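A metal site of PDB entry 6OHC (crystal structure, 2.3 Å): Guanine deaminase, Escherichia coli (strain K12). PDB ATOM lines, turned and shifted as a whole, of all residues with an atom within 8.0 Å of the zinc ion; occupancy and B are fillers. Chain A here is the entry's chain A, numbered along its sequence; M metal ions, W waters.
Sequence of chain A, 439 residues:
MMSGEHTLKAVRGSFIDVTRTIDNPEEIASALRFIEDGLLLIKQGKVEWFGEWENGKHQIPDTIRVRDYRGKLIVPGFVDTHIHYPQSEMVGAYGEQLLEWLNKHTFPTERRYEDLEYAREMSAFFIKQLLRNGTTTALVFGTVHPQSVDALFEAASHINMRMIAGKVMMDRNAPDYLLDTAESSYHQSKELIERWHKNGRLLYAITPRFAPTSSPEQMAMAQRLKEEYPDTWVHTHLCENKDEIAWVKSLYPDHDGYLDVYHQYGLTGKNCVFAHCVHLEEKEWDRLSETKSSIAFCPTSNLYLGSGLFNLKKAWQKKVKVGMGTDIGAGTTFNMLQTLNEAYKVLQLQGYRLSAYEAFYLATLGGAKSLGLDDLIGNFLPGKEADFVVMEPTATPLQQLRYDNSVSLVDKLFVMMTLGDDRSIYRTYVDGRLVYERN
The zinc ion is bound by water W1 (2.0 Å), a ring nitrogen (NE2) of His 82 (2.0 Å), a ring nitrogen (NE2) of His 84 (2.0 Å), a ring nitrogen (NE2) of His 237 (2.1 Å) and the side-chain carboxylate of Asp 327 (2.3 Å). The zinc ion has five donor atoms within binding distance.
The side-chain amide nitrogen of Gln 87 sits at hydrogen-bond distance from a ring nitrogen (ND1) of His 84 (3.3 Å). The side-chain carboxylate of Asp 327 sits at hydrogen-bond distance from the side-chain hydroxyl of Ser 301, at 2.8 Å. A ring nitrogen (ND1) of His 237 lies within hydrogen-bond range of the backbone carbonyl oxygen (O) of Arg 209 (2.9 Å). The backbone NH (N) of His 84 sits close to the backbone carbonyl oxygen (O) of Ile 328. N of Thr 326 sits at hydrogen-bond distance from O of His 82, 3.2 Å away. OD2 of Asp 327 lies close to NE2 of His 276 (3.4 Å). ND1 of His 82 is in hydrogen-bond range of NE2 of His 235 (2.8 Å).
Within 4 Å of the zinc ion: His 82, His 84, His 237 and Asp 327. The nearest printed residue that does not touch the zinc ion is His 276 (4.1 Å).
Water W1 lies within hydrogen-bond range of NE2 of His 276 (3.0 Å) and OD2 of Asp 327 (3.0 Å).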
ATOM      1  N   HIS A  82     -10.064 -24.808   0.340  1.00  0.00           N
ATOM      2  CA  HIS A  82     -11.108 -25.778  -0.057  1.00  0.00           C
ATOM      3  C   HIS A  82     -12.163 -25.071  -0.924  1.00  0.00           C
ATOM      4  O   HIS A  82     -12.943 -24.252  -0.361  1.00  0.00           O
ATOM      5  CB  HIS A  82     -11.707 -26.508   1.153  1.00  0.00           C
ATOM      6  CG  HIS A  82     -12.645 -27.592   0.739  1.00  0.00           C
ATOM      7  ND1 HIS A  82     -12.206 -28.794   0.270  1.00  0.00           N
ATOM      8  CD2 HIS A  82     -13.979 -27.655   0.667  1.00  0.00           C
ATOM      9  CE1 HIS A  82     -13.242 -29.545  -0.026  1.00  0.00           C
ATOM     10  NE2 HIS A  82     -14.317 -28.892   0.209  1.00  0.00           N
ATOM     11  N   ILE A  83     -12.181 -25.393  -2.203  1.00  0.00           N
ATOM     12  CA  ILE A  83     -13.207 -24.914  -3.170  1.00  0.00           C
ATOM     13  C   ILE A  83     -13.448 -25.998  -4.245  1.00  0.00           C
ATOM     14  O   ILE A  83     -12.478 -26.695  -4.622  1.00  0.00           O
ATOM     15  CB  ILE A  83     -12.779 -23.535  -3.713  1.00  0.00           C
ATOM     16  CG1 ILE A  83     -13.930 -22.845  -4.451  1.00  0.00           C
ATOM     17  CG2 ILE A  83     -11.518 -23.570  -4.525  1.00  0.00           C
ATOM     18  CD1 ILE A  83     -13.559 -21.466  -4.998  1.00  0.00           C
ATOM     19  N   HIS A  84     -14.689 -26.136  -4.681  1.00  0.00           N
ATOM     20  CA  HIS A  84     -15.145 -27.029  -5.767  1.00  0.00           C
ATOM     21  C   HIS A  84     -15.312 -26.189  -7.039  1.00  0.00           C
ATOM     22  O   HIS A  84     -16.240 -25.363  -7.103  1.00  0.00           O
ATOM     23  CB  HIS A  84     -16.471 -27.712  -5.406  1.00  0.00           C
ATOM     24  CG  HIS A  84     -16.417 -28.582  -4.196  1.00  0.00           C
ATOM     25  ND1 HIS A  84     -16.294 -29.934  -4.262  1.00  0.00           N
ATOM     26  CD2 HIS A  84     -16.435 -28.260  -2.880  1.00  0.00           C
ATOM     27  CE1 HIS A  84     -16.253 -30.429  -3.048  1.00  0.00           C
ATOM     28  NE2 HIS A  84     -16.376 -29.398  -2.162  1.00  0.00           N
ATOM     29  N   GLN A  87     -19.003 -26.280  -9.303  1.00  0.00           N
ATOM     30  CA  GLN A  87     -20.202 -25.963  -8.478  1.00  0.00           C
ATOM     31  C   GLN A  87     -20.449 -24.435  -8.411  1.00  0.00           C
ATOM     32  O   GLN A  87     -21.254 -24.058  -7.587  1.00  0.00           O
ATOM     33  CB  GLN A  87     -20.044 -26.510  -7.052  1.00  0.00           C
ATOM     34  CG  GLN A  87     -19.834 -28.011  -6.976  1.00  0.00           C
ATOM     35  CD  GLN A  87     -19.729 -28.537  -5.565  1.00  0.00           C
ATOM     36  OE1 GLN A  87     -19.892 -27.773  -4.653  1.00  0.00           O
ATOM     37  NE2 GLN A  87     -19.421 -29.806  -5.380  1.00  0.00           N
ATOM     38  N   THR A 106     -25.362 -31.291  -5.535  1.00  0.00           N
ATOM     39  CA  THR A 106     -23.936 -31.506  -5.884  1.00  0.00           C
ATOM     40  C   THR A 106     -23.847 -32.376  -7.156  1.00  0.00           C
ATOM     41  O   THR A 106     -23.356 -31.909  -8.206  1.00  0.00           O
ATOM     42  CB  THR A 106     -23.218 -32.045  -4.648  1.00  0.00           C
ATOM     43  OG1 THR A 106     -23.600 -31.216  -3.526  1.00  0.00           O
ATOM     44  CG2 THR A 106     -21.718 -32.082  -4.790  1.00  0.00           C
ATOM     45  N   GLU A 110     -22.559 -31.260 -10.926  1.00  0.00           N
ATOM     46  CA  GLU A 110     -21.229 -31.772 -11.379  1.00  0.00           C
ATOM     47  C   GLU A 110     -21.367 -32.542 -12.688  1.00  0.00           C
ATOM     48  O   GLU A 110     -20.403 -32.541 -13.459  1.00  0.00           O
ATOM     49  CB  GLU A 110     -20.567 -32.615 -10.286  1.00  0.00           C
ATOM     50  CG  GLU A 110     -20.249 -31.754  -9.080  1.00  0.00           C
ATOM     51  CD  GLU A 110     -19.222 -32.337  -8.171  1.00  0.00           C
ATOM     52  OE1 GLU A 110     -18.757 -33.410  -8.517  1.00  0.00           O
ATOM     53  OE2 GLU A 110     -18.913 -31.693  -7.136  1.00  0.00           O
ATOM     54  N   PHE A 141     -11.126 -28.943  -5.534  1.00  0.00           N
ATOM     55  CA  PHE A 141     -11.888 -30.126  -5.999  1.00  0.00           C
ATOM     56  C   PHE A 141     -12.266 -29.991  -7.470  1.00  0.00           C
ATOM     57  O   PHE A 141     -12.971 -29.045  -7.829  1.00  0.00           O
ATOM     58  CB  PHE A 141     -13.188 -30.298  -5.225  1.00  0.00           C
ATOM     59  CG  PHE A 141     -13.095 -31.424  -4.234  1.00  0.00           C
ATOM     60  CD1 PHE A 141     -12.213 -31.321  -3.168  1.00  0.00           C
ATOM     61  CD2 PHE A 141     -13.894 -32.539  -4.364  1.00  0.00           C
ATOM     62  CE1 PHE A 141     -12.162 -32.304  -2.226  1.00  0.00           C
ATOM     63  CE2 PHE A 141     -13.835 -33.535  -3.414  1.00  0.00           C
ATOM     64  CZ  PHE A 141     -12.953 -33.421  -2.367  1.00  0.00           C
ATOM     65  N   ARG A 209     -13.399 -38.033  -3.025  1.00  0.00           N
ATOM     66  CA  ARG A 209     -14.476 -37.157  -2.548  1.00  0.00           C
ATOM     67  C   ARG A 209     -14.541 -37.264  -1.032  1.00  0.00           C
ATOM     68  O   ARG A 209     -14.485 -36.159  -0.350  1.00  0.00           O
ATOM     69  CB  ARG A 209     -15.835 -37.449  -3.183  1.00  0.00           C
ATOM     70  CG  ARG A 209     -16.801 -36.326  -2.835  1.00  0.00           C
ATOM     71  CD  ARG A 209     -18.172 -36.367  -3.467  1.00  0.00           C
ATOM     72  NE  ARG A 209     -17.969 -36.182  -4.895  1.00  0.00           N
ATOM     73  CZ  ARG A 209     -18.118 -35.052  -5.586  1.00  0.00           C
ATOM     74  NH1 ARG A 209     -18.516 -33.928  -4.986  1.00  0.00           N
ATOM     75  NH2 ARG A 209     -17.902 -35.059  -6.880  1.00  0.00           N
ATOM     76  N   HIS A 235      -6.350 -34.458  -0.545  1.00  0.00           N
ATOM     77  CA  HIS A 235      -7.453 -33.499  -0.329  1.00  0.00           C
ATOM     78  C   HIS A 235      -8.770 -34.271  -0.222  1.00  0.00           C
ATOM     79  O   HIS A 235      -9.190 -34.807  -1.232  1.00  0.00           O
ATOM     80  CB  HIS A 235      -7.429 -32.474  -1.463  1.00  0.00           C
ATOM     81  CG  HIS A 235      -8.385 -31.361  -1.289  1.00  0.00           C
ATOM     82  ND1 HIS A 235      -8.855 -30.660  -2.343  1.00  0.00           N
ATOM     83  CD2 HIS A 235      -8.927 -30.821  -0.160  1.00  0.00           C
ATOM     84  CE1 HIS A 235      -9.674 -29.732  -1.899  1.00  0.00           C
ATOM     85  NE2 HIS A 235      -9.737 -29.820  -0.550  1.00  0.00           N
ATOM     86  N   THR A 236      -9.381 -34.318   0.949  1.00  0.00           N
ATOM     87  CA  THR A 236     -10.693 -34.963   1.121  1.00  0.00           C
ATOM     88  C   THR A 236     -11.519 -34.206   2.177  1.00  0.00           C
ATOM     89  O   THR A 236     -11.037 -33.193   2.649  1.00  0.00           O
ATOM     90  CB  THR A 236     -10.503 -36.452   1.424  1.00  0.00           C
ATOM     91  OG1 THR A 236     -11.755 -37.070   1.197  1.00  0.00           O
ATOM     92  CG2 THR A 236      -9.998 -36.688   2.828  1.00  0.00           C
ATOM     93  N   HIS A 237     -12.754 -34.660   2.425  1.00  0.00           N
ATOM     94  CA  HIS A 237     -13.674 -34.142   3.455  1.00  0.00           C
ATOM     95  C   HIS A 237     -13.520 -34.989   4.729  1.00  0.00           C
ATOM     96  O   HIS A 237     -13.148 -36.153   4.624  1.00  0.00           O
ATOM     97  CB  HIS A 237     -15.095 -34.088   2.900  1.00  0.00           C
ATOM     98  CG  HIS A 237     -15.304 -33.118   1.782  1.00  0.00           C
ATOM     99  ND1 HIS A 237     -15.132 -33.475   0.457  1.00  0.00           N
ATOM    100  CD2 HIS A 237     -15.749 -31.845   1.763  1.00  0.00           C
ATOM    101  CE1 HIS A 237     -15.436 -32.448  -0.312  1.00  0.00           C
ATOM    102  NE2 HIS A 237     -15.823 -31.429   0.465  1.00  0.00           N
ATOM    103  N   GLU A 240     -17.870 -33.373   8.686  1.00  0.00           N
ATOM    104  CA  GLU A 240     -18.600 -32.113   8.430  1.00  0.00           C
ATOM    105  C   GLU A 240     -19.907 -32.140   9.248  1.00  0.00           C
ATOM    106  O   GLU A 240     -20.346 -31.084   9.738  1.00  0.00           O
ATOM    107  CB  GLU A 240     -18.839 -31.944   6.926  1.00  0.00           C
ATOM    108  CG  GLU A 240     -19.634 -30.700   6.534  1.00  0.00           C
ATOM    109  CD  GLU A 240     -19.809 -30.562   5.029  1.00  0.00           C
ATOM    110  OE1 GLU A 240     -19.394 -31.483   4.322  1.00  0.00           O
ATOM    111  OE2 GLU A 240     -20.351 -29.595   4.568  1.00  0.00           O
ATOM    112  N   ALA A 275     -11.151 -31.075   4.831  1.00  0.00           N
ATOM    113  CA  ALA A 275     -12.140 -29.983   4.839  1.00  0.00           C
ATOM    114  C   ALA A 275     -13.117 -30.211   5.985  1.00  0.00           C
ATOM    115  O   ALA A 275     -13.528 -31.354   6.163  1.00  0.00           O
ATOM    116  CB  ALA A 275     -12.873 -29.890   3.524  1.00  0.00           C
ATOM    117  N   HIS A 276     -13.453 -29.123   6.678  1.00  0.00           N
ATOM    118  CA  HIS A 276     -14.553 -28.977   7.649  1.00  0.00           C
ATOM    119  C   HIS A 276     -14.065 -29.267   9.069  1.00  0.00           C
ATOM    120  O   HIS A 276     -13.873 -28.295   9.836  1.00  0.00           O
ATOM    121  CB  HIS A 276     -15.792 -29.774   7.266  1.00  0.00           C
ATOM    122  CG  HIS A 276     -16.344 -29.384   5.947  1.00  0.00           C
ATOM    123  ND1 HIS A 276     -16.870 -28.123   5.728  1.00  0.00           N
ATOM    124  CD2 HIS A 276     -16.391 -30.066   4.780  1.00  0.00           C
ATOM    125  CE1 HIS A 276     -17.218 -28.030   4.469  1.00  0.00           C
ATOM    126  NE2 HIS A 276     -16.957 -29.233   3.851  1.00  0.00           N
ATOM    127  N   CYS A 298     -14.237 -23.995   6.865  1.00  0.00           N
ATOM    128  CA  CYS A 298     -15.210 -23.573   5.825  1.00  0.00           C
ATOM    129  C   CYS A 298     -16.445 -23.025   6.492  1.00  0.00           C
ATOM    130  O   CYS A 298     -17.525 -23.609   6.438  1.00  0.00           O
ATOM    131  CB  CYS A 298     -15.569 -24.734   4.902  1.00  0.00           C
ATOM    132  SG  CYS A 298     -14.112 -25.397   4.027  1.00  0.00           S
ATOM    133  N   SER A 301     -20.132 -22.558   4.452  1.00  0.00           N
ATOM    134  CA  SER A 301     -20.911 -23.804   4.239  1.00  0.00           C
ATOM    135  C   SER A 301     -21.315 -24.357   5.584  1.00  0.00           C
ATOM    136  O   SER A 301     -22.422 -24.852   5.702  1.00  0.00           O
ATOM    137  CB  SER A 301     -20.198 -24.921   3.403  1.00  0.00           C
ATOM    138  OG  SER A 301     -18.905 -25.087   3.874  1.00  0.00           O
ATOM    139  N   THR A 326     -13.637 -21.461   1.080  1.00  0.00           N
ATOM    140  CA  THR A 326     -14.972 -20.944   0.676  1.00  0.00           C
ATOM    141  C   THR A 326     -15.965 -22.096   0.515  1.00  0.00           C
ATOM    142  O   THR A 326     -17.135 -21.874   0.735  1.00  0.00           O
ATOM    143  CB  THR A 326     -14.847 -20.146  -0.631  1.00  0.00           C
ATOM    144  OG1 THR A 326     -14.325 -20.993  -1.670  1.00  0.00           O
ATOM    145  CG2 THR A 326     -13.962 -18.933  -0.426  1.00  0.00           C
ATOM    146  N   ASP A 327     -15.511 -23.281   0.183  1.00  0.00           N
ATOM    147  CA  ASP A 327     -16.336 -24.479  -0.131  1.00  0.00           C
ATOM    148  C   ASP A 327     -17.453 -24.049  -1.064  1.00  0.00           C
ATOM    149  O   ASP A 327     -18.582 -24.465  -0.907  1.00  0.00           O
ATOM    150  CB  ASP A 327     -16.827 -25.189   1.132  1.00  0.00           C
ATOM    151  CG  ASP A 327     -17.484 -26.547   0.913  1.00  0.00           C
ATOM    152  OD1 ASP A 327     -17.093 -27.319  -0.013  1.00  0.00           O
ATOM    153  OD2 ASP A 327     -18.314 -26.878   1.747  1.00  0.00           O
ATOM    154  N   ILE A 328     -17.122 -23.235  -2.049  1.00  0.00           N
ATOM    155  CA  ILE A 328     -18.016 -22.885  -3.160  1.00  0.00           C
ATOM    156  C   ILE A 328     -18.566 -24.208  -3.687  1.00  0.00           C
ATOM    157  O   ILE A 328     -17.788 -25.174  -3.830  1.00  0.00           O
ATOM    158  CB  ILE A 328     -17.385 -22.068  -4.323  1.00  0.00           C
ATOM    159  CG1 ILE A 328     -17.373 -20.593  -3.988  1.00  0.00           C
ATOM    160  CG2 ILE A 328     -18.068 -22.333  -5.663  1.00  0.00           C
ATOM    161  CD1 ILE A 328     -18.747 -19.931  -4.065  1.00  0.00           C
ATOM    162  N   GLY A 329     -19.805 -24.018  -4.135  1.00  0.00           N
ATOM    163  CA  GLY A 329     -20.945 -24.897  -4.041  1.00  0.00           C
ATOM    164  C   GLY A 329     -21.752 -24.523  -2.836  1.00  0.00           C
ATOM    165  O   GLY A 329     -22.696 -23.778  -2.990  1.00  0.00           O
ATOM    166  N   ALA A 330     -21.390 -25.160  -1.721  1.00  0.00           N
ATOM    167  CA  ALA A 330     -22.171 -25.176  -0.481  1.00  0.00           C
ATOM    168  C   ALA A 330     -22.091 -23.788   0.178  1.00  0.00           C
ATOM    169  O   ALA A 330     -23.045 -23.365   0.751  1.00  0.00           O
ATOM    170  CB  ALA A 330     -21.611 -26.292   0.351  1.00  0.00           C
ATOM    171  N   GLY A 331     -20.929 -23.157   0.106  1.00  0.00           N
ATOM    172  CA  GLY A 331     -20.674 -21.769   0.469  1.00  0.00           C
ATOM    173  C   GLY A 331     -21.099 -20.885  -0.677  1.00  0.00           C
ATOM    174  O   GLY A 331     -21.050 -21.374  -1.799  1.00  0.00           O
HETATM  175 ZN    ZN M   1     -16.206 -29.446  -0.157  1.00  0.00          ZN
HETATM  176  O   HOH W   1     -17.762 -29.772   1.037  1.00  0.00           O
